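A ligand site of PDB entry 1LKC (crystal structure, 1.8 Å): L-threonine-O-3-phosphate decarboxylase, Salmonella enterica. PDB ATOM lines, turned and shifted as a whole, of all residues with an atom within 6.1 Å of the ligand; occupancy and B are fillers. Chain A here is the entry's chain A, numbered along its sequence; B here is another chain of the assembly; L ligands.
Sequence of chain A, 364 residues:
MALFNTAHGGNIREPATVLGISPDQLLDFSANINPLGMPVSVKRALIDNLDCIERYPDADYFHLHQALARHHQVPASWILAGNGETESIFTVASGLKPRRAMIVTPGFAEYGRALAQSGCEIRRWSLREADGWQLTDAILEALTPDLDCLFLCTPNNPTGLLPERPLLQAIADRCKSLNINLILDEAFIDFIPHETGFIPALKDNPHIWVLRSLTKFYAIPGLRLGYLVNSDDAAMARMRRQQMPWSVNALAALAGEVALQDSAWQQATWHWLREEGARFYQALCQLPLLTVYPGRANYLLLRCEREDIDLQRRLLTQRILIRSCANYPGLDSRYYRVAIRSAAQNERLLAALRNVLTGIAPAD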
ATOM      1  N   ASN A  83      -1.787   7.304 -27.233  1.00  0.00           N
ATOM      2  CA  ASN A  83      -0.457   7.949 -27.248  1.00  0.00           C
ATOM      3  C   ASN A  83      -0.133   8.078 -25.739  1.00  0.00           C
ATOM      4  O   ASN A  83      -0.189   9.193 -25.169  1.00  0.00           O
ATOM      5  CB  ASN A  83      -0.602   9.322 -27.915  1.00  0.00           C
ATOM      6  CG  ASN A  83       0.688  10.098 -28.017  1.00  0.00           C
ATOM      7  OD1 ASN A  83       0.715  11.347 -27.844  1.00  0.00           O
ATOM      8  ND2 ASN A  83       1.747   9.412 -28.348  1.00  0.00           N
ATOM      9  N   GLY A  84       0.243   6.938 -25.144  1.00  0.00           N
ATOM     10  CA  GLY A  84       0.476   6.834 -23.714  1.00  0.00           C
ATOM     11  C   GLY A  84      -0.866   6.524 -23.052  1.00  0.00           C
ATOM     12  O   GLY A  84      -1.935   6.842 -23.596  1.00  0.00           O
ATOM     13  N   GLU A  85      -0.853   5.842 -21.894  1.00  0.00           N
ATOM     14  CA  GLU A  85      -2.136   5.632 -21.179  1.00  0.00           C
ATOM     15  C   GLU A  85      -2.757   7.025 -20.842  1.00  0.00           C
ATOM     16  O   GLU A  85      -3.962   7.183 -20.638  1.00  0.00           O
ATOM     17  CB  GLU A  85      -1.884   4.910 -19.873  1.00  0.00           C
ATOM     18  CG  GLU A  85      -3.225   4.455 -19.260  1.00  0.00           C
ATOM     19  CD  GLU A  85      -3.043   3.868 -17.884  1.00  0.00           C
ATOM     20  OE1 GLU A  85      -2.408   2.810 -17.785  1.00  0.00           O
ATOM     21  OE2 GLU A  85      -3.560   4.469 -16.906  1.00  0.00           O
ATOM     22  N   THR A  86      -1.896   8.034 -20.795  1.00  0.00           N
ATOM     23  CA  THR A  86      -2.342   9.391 -20.516  1.00  0.00           C
ATOM     24  C   THR A  86      -3.416   9.760 -21.556  1.00  0.00           C
ATOM     25  O   THR A  86      -4.462  10.361 -21.225  1.00  0.00           O
ATOM     26  CB  THR A  86      -1.158  10.400 -20.632  1.00  0.00           C
ATOM     27  OG1 THR A  86      -0.270  10.185 -19.508  1.00  0.00           O
ATOM     28  CG2 THR A  86      -1.658  11.855 -20.571  1.00  0.00           C
ATOM     29  N   GLU A  87      -3.177   9.436 -22.826  1.00  0.00           N
ATOM     30  CA  GLU A  87      -4.194   9.752 -23.825  1.00  0.00           C
ATOM     31  C   GLU A  87      -5.460   8.971 -23.533  1.00  0.00           C
ATOM     32  O   GLU A  87      -6.565   9.515 -23.619  1.00  0.00           O
ATOM     33  CB  GLU A  87      -3.735   9.450 -25.252  1.00  0.00           C
ATOM     34  CG  GLU A  87      -4.803   9.861 -26.237  1.00  0.00           C
ATOM     35  CD  GLU A  87      -4.335   9.864 -27.664  1.00  0.00           C
ATOM     36  OE1 GLU A  87      -3.825   8.824 -28.126  1.00  0.00           O
ATOM     37  OE2 GLU A  87      -4.484  10.919 -28.329  1.00  0.00           O
ATOM     38  N   ILE A  89      -6.679   8.116 -20.768  1.00  0.00           N
ATOM     39  CA  ILE A  89      -7.413   8.778 -19.652  1.00  0.00           C
ATOM     40  C   ILE A  89      -8.244   9.938 -20.230  1.00  0.00           C
ATOM     41  O   ILE A  89      -9.422  10.098 -19.871  1.00  0.00           O
ATOM     42  CB  ILE A  89      -6.415   9.348 -18.606  1.00  0.00           C
ATOM     43  CG1 ILE A  89      -5.772   8.174 -17.788  1.00  0.00           C
ATOM     44  CG2 ILE A  89      -7.133  10.354 -17.680  1.00  0.00           C
ATOM     45  CD1 ILE A  89      -4.585   8.611 -16.886  1.00  0.00           C
ATOM     46  N   PHE A 108      -3.664   9.754  -8.795  1.00  0.00           N
ATOM     47  CA  PHE A 108      -3.020  10.271  -9.983  1.00  0.00           C
ATOM     48  C   PHE A 108      -3.737  11.568 -10.473  1.00  0.00           C
ATOM     49  O   PHE A 108      -4.908  11.542 -10.767  1.00  0.00           O
ATOM     50  CB  PHE A 108      -3.040   9.172 -11.068  1.00  0.00           C
ATOM     51  CG  PHE A 108      -2.157   9.462 -12.236  1.00  0.00           C
ATOM     52  CD1 PHE A 108      -0.771   9.591 -12.068  1.00  0.00           C
ATOM     53  CD2 PHE A 108      -2.698   9.639 -13.536  1.00  0.00           C
ATOM     54  CE1 PHE A 108       0.062   9.896 -13.162  1.00  0.00           C
ATOM     55  CE2 PHE A 108      -1.870   9.950 -14.618  1.00  0.00           C
ATOM     56  CZ  PHE A 108      -0.488  10.080 -14.426  1.00  0.00           C
ATOM     57  N   TYR A 111      -6.524  12.550 -13.726  1.00  0.00           N
ATOM     58  CA  TYR A 111      -7.978  12.324 -13.800  1.00  0.00           C
ATOM     59  C   TYR A 111      -8.700  13.632 -13.523  1.00  0.00           C
ATOM     60  O   TYR A 111      -9.635  13.976 -14.242  1.00  0.00           O
ATOM     61  CB  TYR A 111      -8.441  11.271 -12.768  1.00  0.00           C
ATOM     62  CG  TYR A 111      -8.047   9.916 -13.247  1.00  0.00           C
ATOM     63  CD1 TYR A 111      -6.826   9.337 -12.860  1.00  0.00           C
ATOM     64  CD2 TYR A 111      -8.779   9.281 -14.239  1.00  0.00           C
ATOM     65  CE1 TYR A 111      -6.350   8.134 -13.483  1.00  0.00           C
ATOM     66  CE2 TYR A 111      -8.322   8.108 -14.861  1.00  0.00           C
ATOM     67  CZ  TYR A 111      -7.115   7.548 -14.472  1.00  0.00           C
ATOM     68  OH  TYR A 111      -6.692   6.407 -15.108  1.00  0.00           O
ATOM     69  N   CYS A 153      -7.380   3.671  -8.929  1.00  0.00           N
ATOM     70  CA  CYS A 153      -6.038   3.382  -9.477  1.00  0.00           C
ATOM     71  C   CYS A 153      -5.684   2.058  -8.790  1.00  0.00           C
ATOM     72  O   CYS A 153      -5.642   2.009  -7.565  1.00  0.00           O
ATOM     73  CB  CYS A 153      -5.089   4.451  -9.003  1.00  0.00           C
ATOM     74  SG  CYS A 153      -3.684   4.625 -10.008  1.00  0.00           S
ATOM     75  N   PRO A 155      -2.667  -0.779  -8.817  1.00  0.00           N
ATOM     76  CA  PRO A 155      -2.456  -0.202  -7.486  1.00  0.00           C
ATOM     77  C   PRO A 155      -2.479   1.335  -7.540  1.00  0.00           C
ATOM     78  O   PRO A 155      -2.311   1.938  -8.594  1.00  0.00           O
ATOM     79  CB  PRO A 155      -1.064  -0.710  -7.122  1.00  0.00           C
ATOM     80  CG  PRO A 155      -0.357  -0.657  -8.407  1.00  0.00           C
ATOM     81  CD  PRO A 155      -1.414  -1.282  -9.360  1.00  0.00           C
ATOM     82  N   ASN A 156      -2.600   1.940  -6.369  1.00  0.00           N
ATOM     83  CA  ASN A 156      -2.676   3.410  -6.297  1.00  0.00           C
ATOM     84  C   ASN A 156      -1.322   4.078  -6.493  1.00  0.00           C
ATOM     85  O   ASN A 156      -0.295   3.523  -6.160  1.00  0.00           O
ATOM     86  CB  ASN A 156      -3.256   3.822  -4.952  1.00  0.00           C
ATOM     87  CG  ASN A 156      -3.859   5.219  -5.001  1.00  0.00           C
ATOM     88  OD1 ASN A 156      -4.018   5.805  -6.087  1.00  0.00           O
ATOM     89  ND2 ASN A 156      -4.224   5.733  -3.849  1.00  0.00           N
ATOM     90  N   ASN A 157      -1.344   5.256  -7.118  1.00  0.00           N
ATOM     91  CA  ASN A 157      -0.128   6.037  -7.344  1.00  0.00           C
ATOM     92  C   ASN A 157      -0.561   7.264  -6.555  1.00  0.00           C
ATOM     93  O   ASN A 157      -1.524   7.908  -6.946  1.00  0.00           O
ATOM     94  CB  ASN A 157       0.035   6.354  -8.848  1.00  0.00           C
ATOM     95  CG  ASN A 157       1.203   7.251  -9.122  1.00  0.00           C
ATOM     96  OD1 ASN A 157       1.667   7.933  -8.200  1.00  0.00           O
ATOM     97  ND2 ASN A 157       1.659   7.309 -10.389  1.00  0.00           N
ATOM     98  N   ASP A 185      -7.479   2.055 -13.249  1.00  0.00           N
ATOM     99  CA  ASP A 185      -6.207   2.357 -13.856  1.00  0.00           C
ATOM    100  C   ASP A 185      -5.185   1.300 -13.404  1.00  0.00           C
ATOM    101  O   ASP A 185      -4.693   1.323 -12.258  1.00  0.00           O
ATOM    102  CB  ASP A 185      -5.781   3.759 -13.400  1.00  0.00           C
ATOM    103  CG  ASP A 185      -4.529   4.252 -14.094  1.00  0.00           C
ATOM    104  OD1 ASP A 185      -3.723   3.378 -14.497  1.00  0.00           O
ATOM    105  OD2 ASP A 185      -4.360   5.487 -14.224  1.00  0.00           O
ATOM    106  N   ALA A 187      -2.112   0.796 -14.697  1.00  0.00           N
ATOM    107  CA  ALA A 187      -0.798   1.133 -15.196  1.00  0.00           C
ATOM    108  C   ALA A 187       0.338   0.274 -14.647  1.00  0.00           C
ATOM    109  O   ALA A 187       1.300  -0.073 -15.361  1.00  0.00           O
ATOM    110  CB  ALA A 187      -0.480   2.633 -14.869  1.00  0.00           C
ATOM    111  N   PHE A 188       0.248  -0.078 -13.368  1.00  0.00           N
ATOM    112  CA  PHE A 188       1.364  -0.843 -12.741  1.00  0.00           C
ATOM    113  C   PHE A 188       0.966  -2.273 -12.381  1.00  0.00           C
ATOM    114  O   PHE A 188       1.743  -2.974 -11.742  1.00  0.00           O
ATOM    115  CB  PHE A 188       1.769  -0.150 -11.440  1.00  0.00           C
ATOM    116  CG  PHE A 188       2.502   1.148 -11.642  1.00  0.00           C
ATOM    117  CD1 PHE A 188       1.837   2.354 -11.569  1.00  0.00           C
ATOM    118  CD2 PHE A 188       3.857   1.143 -11.855  1.00  0.00           C
ATOM    119  CE1 PHE A 188       2.516   3.535 -11.711  1.00  0.00           C
ATOM    120  CE2 PHE A 188       4.569   2.322 -12.000  1.00  0.00           C
ATOM    121  CZ  PHE A 188       3.879   3.541 -11.918  1.00  0.00           C
ATOM    122  N   ARG A 212      -4.444   0.635 -19.421  1.00  0.00           N
ATOM    123  CA  ARG A 212      -3.168  -0.026 -19.308  1.00  0.00           C
ATOM    124  C   ARG A 212      -2.091   0.846 -19.893  1.00  0.00           C
ATOM    125  O   ARG A 212      -2.342   1.656 -20.762  1.00  0.00           O
ATOM    126  CB  ARG A 212      -3.173  -1.317 -20.103  1.00  0.00           C
ATOM    127  CG  ARG A 212      -4.080  -2.422 -19.556  1.00  0.00           C
ATOM    128  CD  ARG A 212      -3.781  -2.667 -18.091  1.00  0.00           C
ATOM    129  NE  ARG A 212      -4.145  -4.011 -17.620  1.00  0.00           N
ATOM    130  CZ  ARG A 212      -3.345  -5.069 -17.704  1.00  0.00           C
ATOM    131  NH1 ARG A 212      -2.143  -4.957 -18.252  1.00  0.00           N
ATOM    132  NH2 ARG A 212      -3.764  -6.247 -17.276  1.00  0.00           N
ATOM    133  N   SER A 213      -0.852   0.631 -19.467  1.00  0.00           N
ATOM    134  CA  SER A 213       0.244   1.390 -20.026  1.00  0.00           C
ATOM    135  C   SER A 213       1.405   0.442 -20.302  1.00  0.00           C
ATOM    136  O   SER A 213       1.619  -0.484 -19.503  1.00  0.00           O
ATOM    137  CB  SER A 213       0.771   2.358 -18.980  1.00  0.00           C
ATOM    138  OG  SER A 213       1.846   3.064 -19.551  1.00  0.00           O
ATOM    139  N   LEU A 214       2.120   0.665 -21.405  1.00  0.00           N
ATOM    140  CA  LEU A 214       3.369  -0.120 -21.643  1.00  0.00           C
ATOM    141  C   LEU A 214       4.576   0.690 -21.149  1.00  0.00           C
ATOM    142  O   LEU A 214       5.716   0.193 -21.144  1.00  0.00           O
ATOM    143  CB  LEU A 214       3.608  -0.424 -23.128  1.00  0.00           C
ATOM    144  CG  LEU A 214       2.774  -1.561 -23.716  1.00  0.00           C
ATOM    145  CD1 LEU A 214       1.387  -1.065 -24.046  1.00  0.00           C
ATOM    146  CD2 LEU A 214       3.460  -2.098 -25.003  1.00  0.00           C
ATOM    147  N   THR A 215       4.329   1.925 -20.709  1.00  0.00           N
ATOM    148  CA  THR A 215       5.367   2.821 -20.260  1.00  0.00           C
ATOM    149  C   THR A 215       6.311   2.347 -19.153  1.00  0.00           C
ATOM    150  O   THR A 215       7.540   2.343 -19.321  1.00  0.00           O
ATOM    151  CB  THR A 215       4.754   4.195 -19.757  1.00  0.00           C
ATOM    152  OG1 THR A 215       4.417   4.968 -20.903  1.00  0.00           O
ATOM    153  CG2 THR A 215       5.782   4.970 -18.922  1.00  0.00           C
ATOM    154  N   LYS A 216       5.739   1.937 -18.028  1.00  0.00           N
ATOM    155  CA  LYS A 216       6.576   1.552 -16.892  1.00  0.00           C
ATOM    156  C   LYS A 216       7.066   0.141 -17.057  1.00  0.00           C
ATOM    157  O   LYS A 216       8.257  -0.136 -16.931  1.00  0.00           O
ATOM    158  CB  LYS A 216       5.803   1.649 -15.586  1.00  0.00           C
ATOM    159  CG  LYS A 216       5.672   3.097 -15.064  1.00  0.00           C
ATOM    160  CD  LYS A 216       4.519   3.797 -15.661  1.00  0.00           C
ATOM    161  CE  LYS A 216       4.454   5.322 -15.283  1.00  0.00           C
ATOM    162  NZ  LYS A 216       3.011   5.547 -15.156  1.00  0.00           N
ATOM    163  N   PRO A 221       8.752   4.730 -21.869  1.00  0.00           N
ATOM    164  CA  PRO A 221       8.032   6.006 -21.642  1.00  0.00           C
ATOM    165  C   PRO A 221       8.214   7.035 -22.735  1.00  0.00           C
ATOM    166  O   PRO A 221       7.302   7.833 -22.969  1.00  0.00           O
ATOM    167  CB  PRO A 221       8.619   6.525 -20.329  1.00  0.00           C
ATOM    168  CG  PRO A 221      10.020   5.973 -20.337  1.00  0.00           C
ATOM    169  CD  PRO A 221       9.717   4.520 -20.769  1.00  0.00           C
ATOM    170  N   ARG A 224       5.636   6.514 -25.889  1.00  0.00           N
ATOM    171  CA  ARG A 224       4.220   6.758 -25.566  1.00  0.00           C
ATOM    172  C   ARG A 224       3.215   5.721 -26.045  1.00  0.00           C
ATOM    173  O   ARG A 224       2.682   5.827 -27.167  1.00  0.00           O
ATOM    174  CB  ARG A 224       3.735   8.132 -26.084  1.00  0.00           C
ATOM    175  CG  ARG A 224       4.749   9.294 -25.924  1.00  0.00           C
ATOM    176  CD  ARG A 224       5.150   9.586 -24.449  1.00  0.00           C
ATOM    177  NE  ARG A 224       3.954   9.872 -23.664  1.00  0.00           N
ATOM    178  CZ  ARG A 224       3.570   9.198 -22.579  1.00  0.00           C
ATOM    179  NH1 ARG A 224       4.290   8.181 -22.104  1.00  0.00           N
ATOM    180  NH2 ARG A 224       2.398   9.506 -22.009  1.00  0.00           N
ATOM    181  N   LEU A 225       2.917   4.743 -25.211  1.00  0.00           N
ATOM    182  CA  LEU A 225       1.929   3.769 -25.599  1.00  0.00           C
ATOM    183  C   LEU A 225       1.145   3.192 -24.415  1.00  0.00           C
ATOM    184  O   LEU A 225       1.708   2.699 -23.436  1.00  0.00           O
ATOM    185  CB  LEU A 225       2.533   2.605 -26.399  1.00  0.00           C
ATOM    186  CG  LEU A 225       1.441   1.669 -26.949  1.00  0.00           C
ATOM    187  CD1 LEU A 225       0.610   2.358 -28.062  1.00  0.00           C
ATOM    188  CD2 LEU A 225       2.158   0.464 -27.589  1.00  0.00           C
ATOM    189  N   GLY A 226      -0.178   3.300 -24.526  1.00  0.00           N
ATOM    190  CA  GLY A 226      -1.060   2.739 -23.525  1.00  0.00           C
ATOM    191  C   GLY A 226      -2.321   2.291 -24.236  1.00  0.00           C
ATOM    192  O   GLY A 226      -2.373   2.373 -25.474  1.00  0.00           O
ATOM    193  N   TYR B  56      11.004   9.360 -19.972  1.00  0.00           N
ATOM    194  CA  TYR B  56       9.942  10.234 -20.467  1.00  0.00           C
ATOM    195  C   TYR B  56      10.547  11.396 -21.273  1.00  0.00           C
ATOM    196  O   TYR B  56      11.692  11.786 -21.043  1.00  0.00           O
ATOM    197  CB  TYR B  56       9.134  10.819 -19.270  1.00  0.00           C
ATOM    198  CG  TYR B  56       7.932  10.002 -18.797  1.00  0.00           C
ATOM    199  CD1 TYR B  56       8.014   9.131 -17.696  1.00  0.00           C
ATOM    200  CD2 TYR B  56       6.720  10.065 -19.469  1.00  0.00           C
ATOM    201  CE1 TYR B  56       6.917   8.328 -17.284  1.00  0.00           C
ATOM    202  CE2 TYR B  56       5.614   9.279 -19.079  1.00  0.00           C
ATOM    203  CZ  TYR B  56       5.720   8.417 -17.990  1.00  0.00           C
ATOM    204  OH  TYR B  56       4.619   7.631 -17.657  1.00  0.00           O
ATOM    205  N   TRP B 246       3.253  15.198 -22.200  1.00  0.00           N
ATOM    206  CA  TRP B 246       4.132  14.271 -22.868  1.00  0.00           C
ATOM    207  C   TRP B 246       3.584  13.847 -24.218  1.00  0.00           C
ATOM    208  O   TRP B 246       3.939  12.794 -24.699  1.00  0.00           O
ATOM    209  CB  TRP B 246       4.285  13.007 -22.028  1.00  0.00           C
ATOM    210  CG  TRP B 246       4.872  13.203 -20.692  1.00  0.00           C
ATOM    211  CD1 TRP B 246       6.111  13.707 -20.394  1.00  0.00           C
ATOM    212  CD2 TRP B 246       4.282  12.799 -19.451  1.00  0.00           C
ATOM    213  NE1 TRP B 246       6.326  13.631 -19.028  1.00  0.00           N
ATOM    214  CE2 TRP B 246       5.225  13.083 -18.433  1.00  0.00           C
ATOM    215  CE3 TRP B 246       3.056  12.231 -19.098  1.00  0.00           C
ATOM    216  CZ2 TRP B 246       4.965  12.814 -17.087  1.00  0.00           C
ATOM    217  CZ3 TRP B 246       2.805  11.958 -17.754  1.00  0.00           C
ATOM    218  CH2 TRP B 246       3.756  12.251 -16.764  1.00  0.00           C
HETATM  219  N1  LIG L   1      -1.749   6.276 -14.706  1.00  0.00           N
HETATM  220  C1  LIG L   1      -0.954   5.978 -13.659  1.00  0.00           C
HETATM  221  C2  LIG L   1      -1.524   5.522 -12.382  1.00  0.00           C
HETATM  222  C3  LIG L   1       0.461   6.138 -13.887  1.00  0.00           C
HETATM  223  O1  LIG L   1       1.267   5.870 -12.928  1.00  0.00           O
HETATM  224  C4  LIG L   1       0.910   6.579 -15.152  1.00  0.00           C
HETATM  225  C5  LIG L   1       2.384   6.688 -15.330  1.00  0.00           C
HETATM  226  C6  LIG L   1      -0.004   6.872 -16.192  1.00  0.00           C
HETATM  227  C7  LIG L   1      -1.365   6.710 -15.941  1.00  0.00           C
HETATM  228  C8  LIG L   1       0.325   7.331 -17.564  1.00  0.00           C
HETATM  229  O2  LIG L   1       1.232   6.442 -18.286  1.00  0.00           O
HETATM  230  P1  LIG L   1       1.679   6.720 -19.794  1.00  0.00           P
HETATM  231  O3  LIG L   1       1.444   5.383 -20.535  1.00  0.00           O
HETATM  232  O4  LIG L   1       3.224   7.014 -19.808  1.00  0.00           O
HETATM  233  O5  LIG L   1       0.906   7.998 -20.244  1.00  0.00           O
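C of Gly 84 touches O3 of the ligand (3.6 Å). CD1 of Ile 89 touches C7 of the ligand, 3.9 Å away. CE2 of Phe 108 touches C7 of the ligand (3.5 Å). Cys 153 touches the ligand (SG to C2, 3.3 Å). CB of Ala 187 touches C1 of the ligand (3.6 Å). CE1 of Phe 188 touches O1 of the ligand, 2.9 Å away. O of Leu 225 touches O3 of the ligand, at 3.96 Å. Hydrophobic or aromatic side chains within 4 Å of the ligand: Ile 89, Phe 108, Ala 187, Phe 188 and Tyr 56 of chain B. 16 residues have an atom within 4 Å of the ligand: Gly 84, Glu 85, Thr 86, Ile 89, Phe 108, Cys 153, Asn 157, Asp 185, Ala 187, Phe 188, Ser 213, Thr 215, Lys 216, Arg 224, Leu 225 and Tyr 56 of chain B.
The side-chain hydroxyl of Thr 215 sits at hydrogen-bond distance from the guanidinium group of Arg 224, at 3.4 Å. The side-chain carboxylate (OE1) of Glu 85 lies close to the backbone NH (N) of Arg 212, 3.4 Å away. The backbone NH (N) of Gly 84 lies close to the backbone carbonyl oxygen (O) of Arg 224 (3.4 Å). The backbone carbonyl oxygen (O) of Leu 225 lies within hydrogen-bond range of the backbone NH (N) of Leu 214 (2.9 Å). The side-chain hydroxyl (OG) of Ser 213 sits at hydrogen-bond distance from the backbone NH (N) of Thr 215, 3.0 Å away. The side-chain carboxylate (OD1) of Asp 185 lies close to the side-chain carboxylate (OE2) of Glu 85 (2.6 Å). N of Ser 213 lies within hydrogen-bond range of OE1 of Glu 85 (3.2 Å). O of Trp 246 of chain B sits at hydrogen-bond distance from NE of Arg 224.
The guanidinium group (NH2) of Arg 224 is in salt-bridge range of an oxygen (O5) of the ligand (2.8 Å). The side-chain hydroxyl (OG) of Ser 213 sits at hydrogen-bond distance from an oxygen (O3) of the ligand, 2.6 Å away. The side-chain amino group (NZ) of Lys 216 is covalently linked to a carbon (C5) of the ligand (1.3 Å). The backbone NH (N) of Thr 86 lies within hydrogen-bond range of an oxygen (O5) of the ligand, at 2.9 Å. OH of Tyr 56 of chain B lies within hydrogen-bond range of O4 of the ligand (2.6 Å). A nitrogen (N1) of the ligand lies within hydrogen-bond range of the side-chain carboxylate of Asp 185 (2.8 Å). OG1 of Thr 215 lies within hydrogen-bond range of O4 of the ligand (2.6 Å). The side-chain amide nitrogen of Asn 157 lies within hydrogen-bond range of an oxygen (O1) of the ligand, 2.9 Å away. The backbone NH (N) of Glu 85 sits at hydrogen-bond distance from an oxygen (O3) of the ligand. OG1 of Thr 86 lies within hydrogen-bond range of O5 of the ligand, at 2.6 Å.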
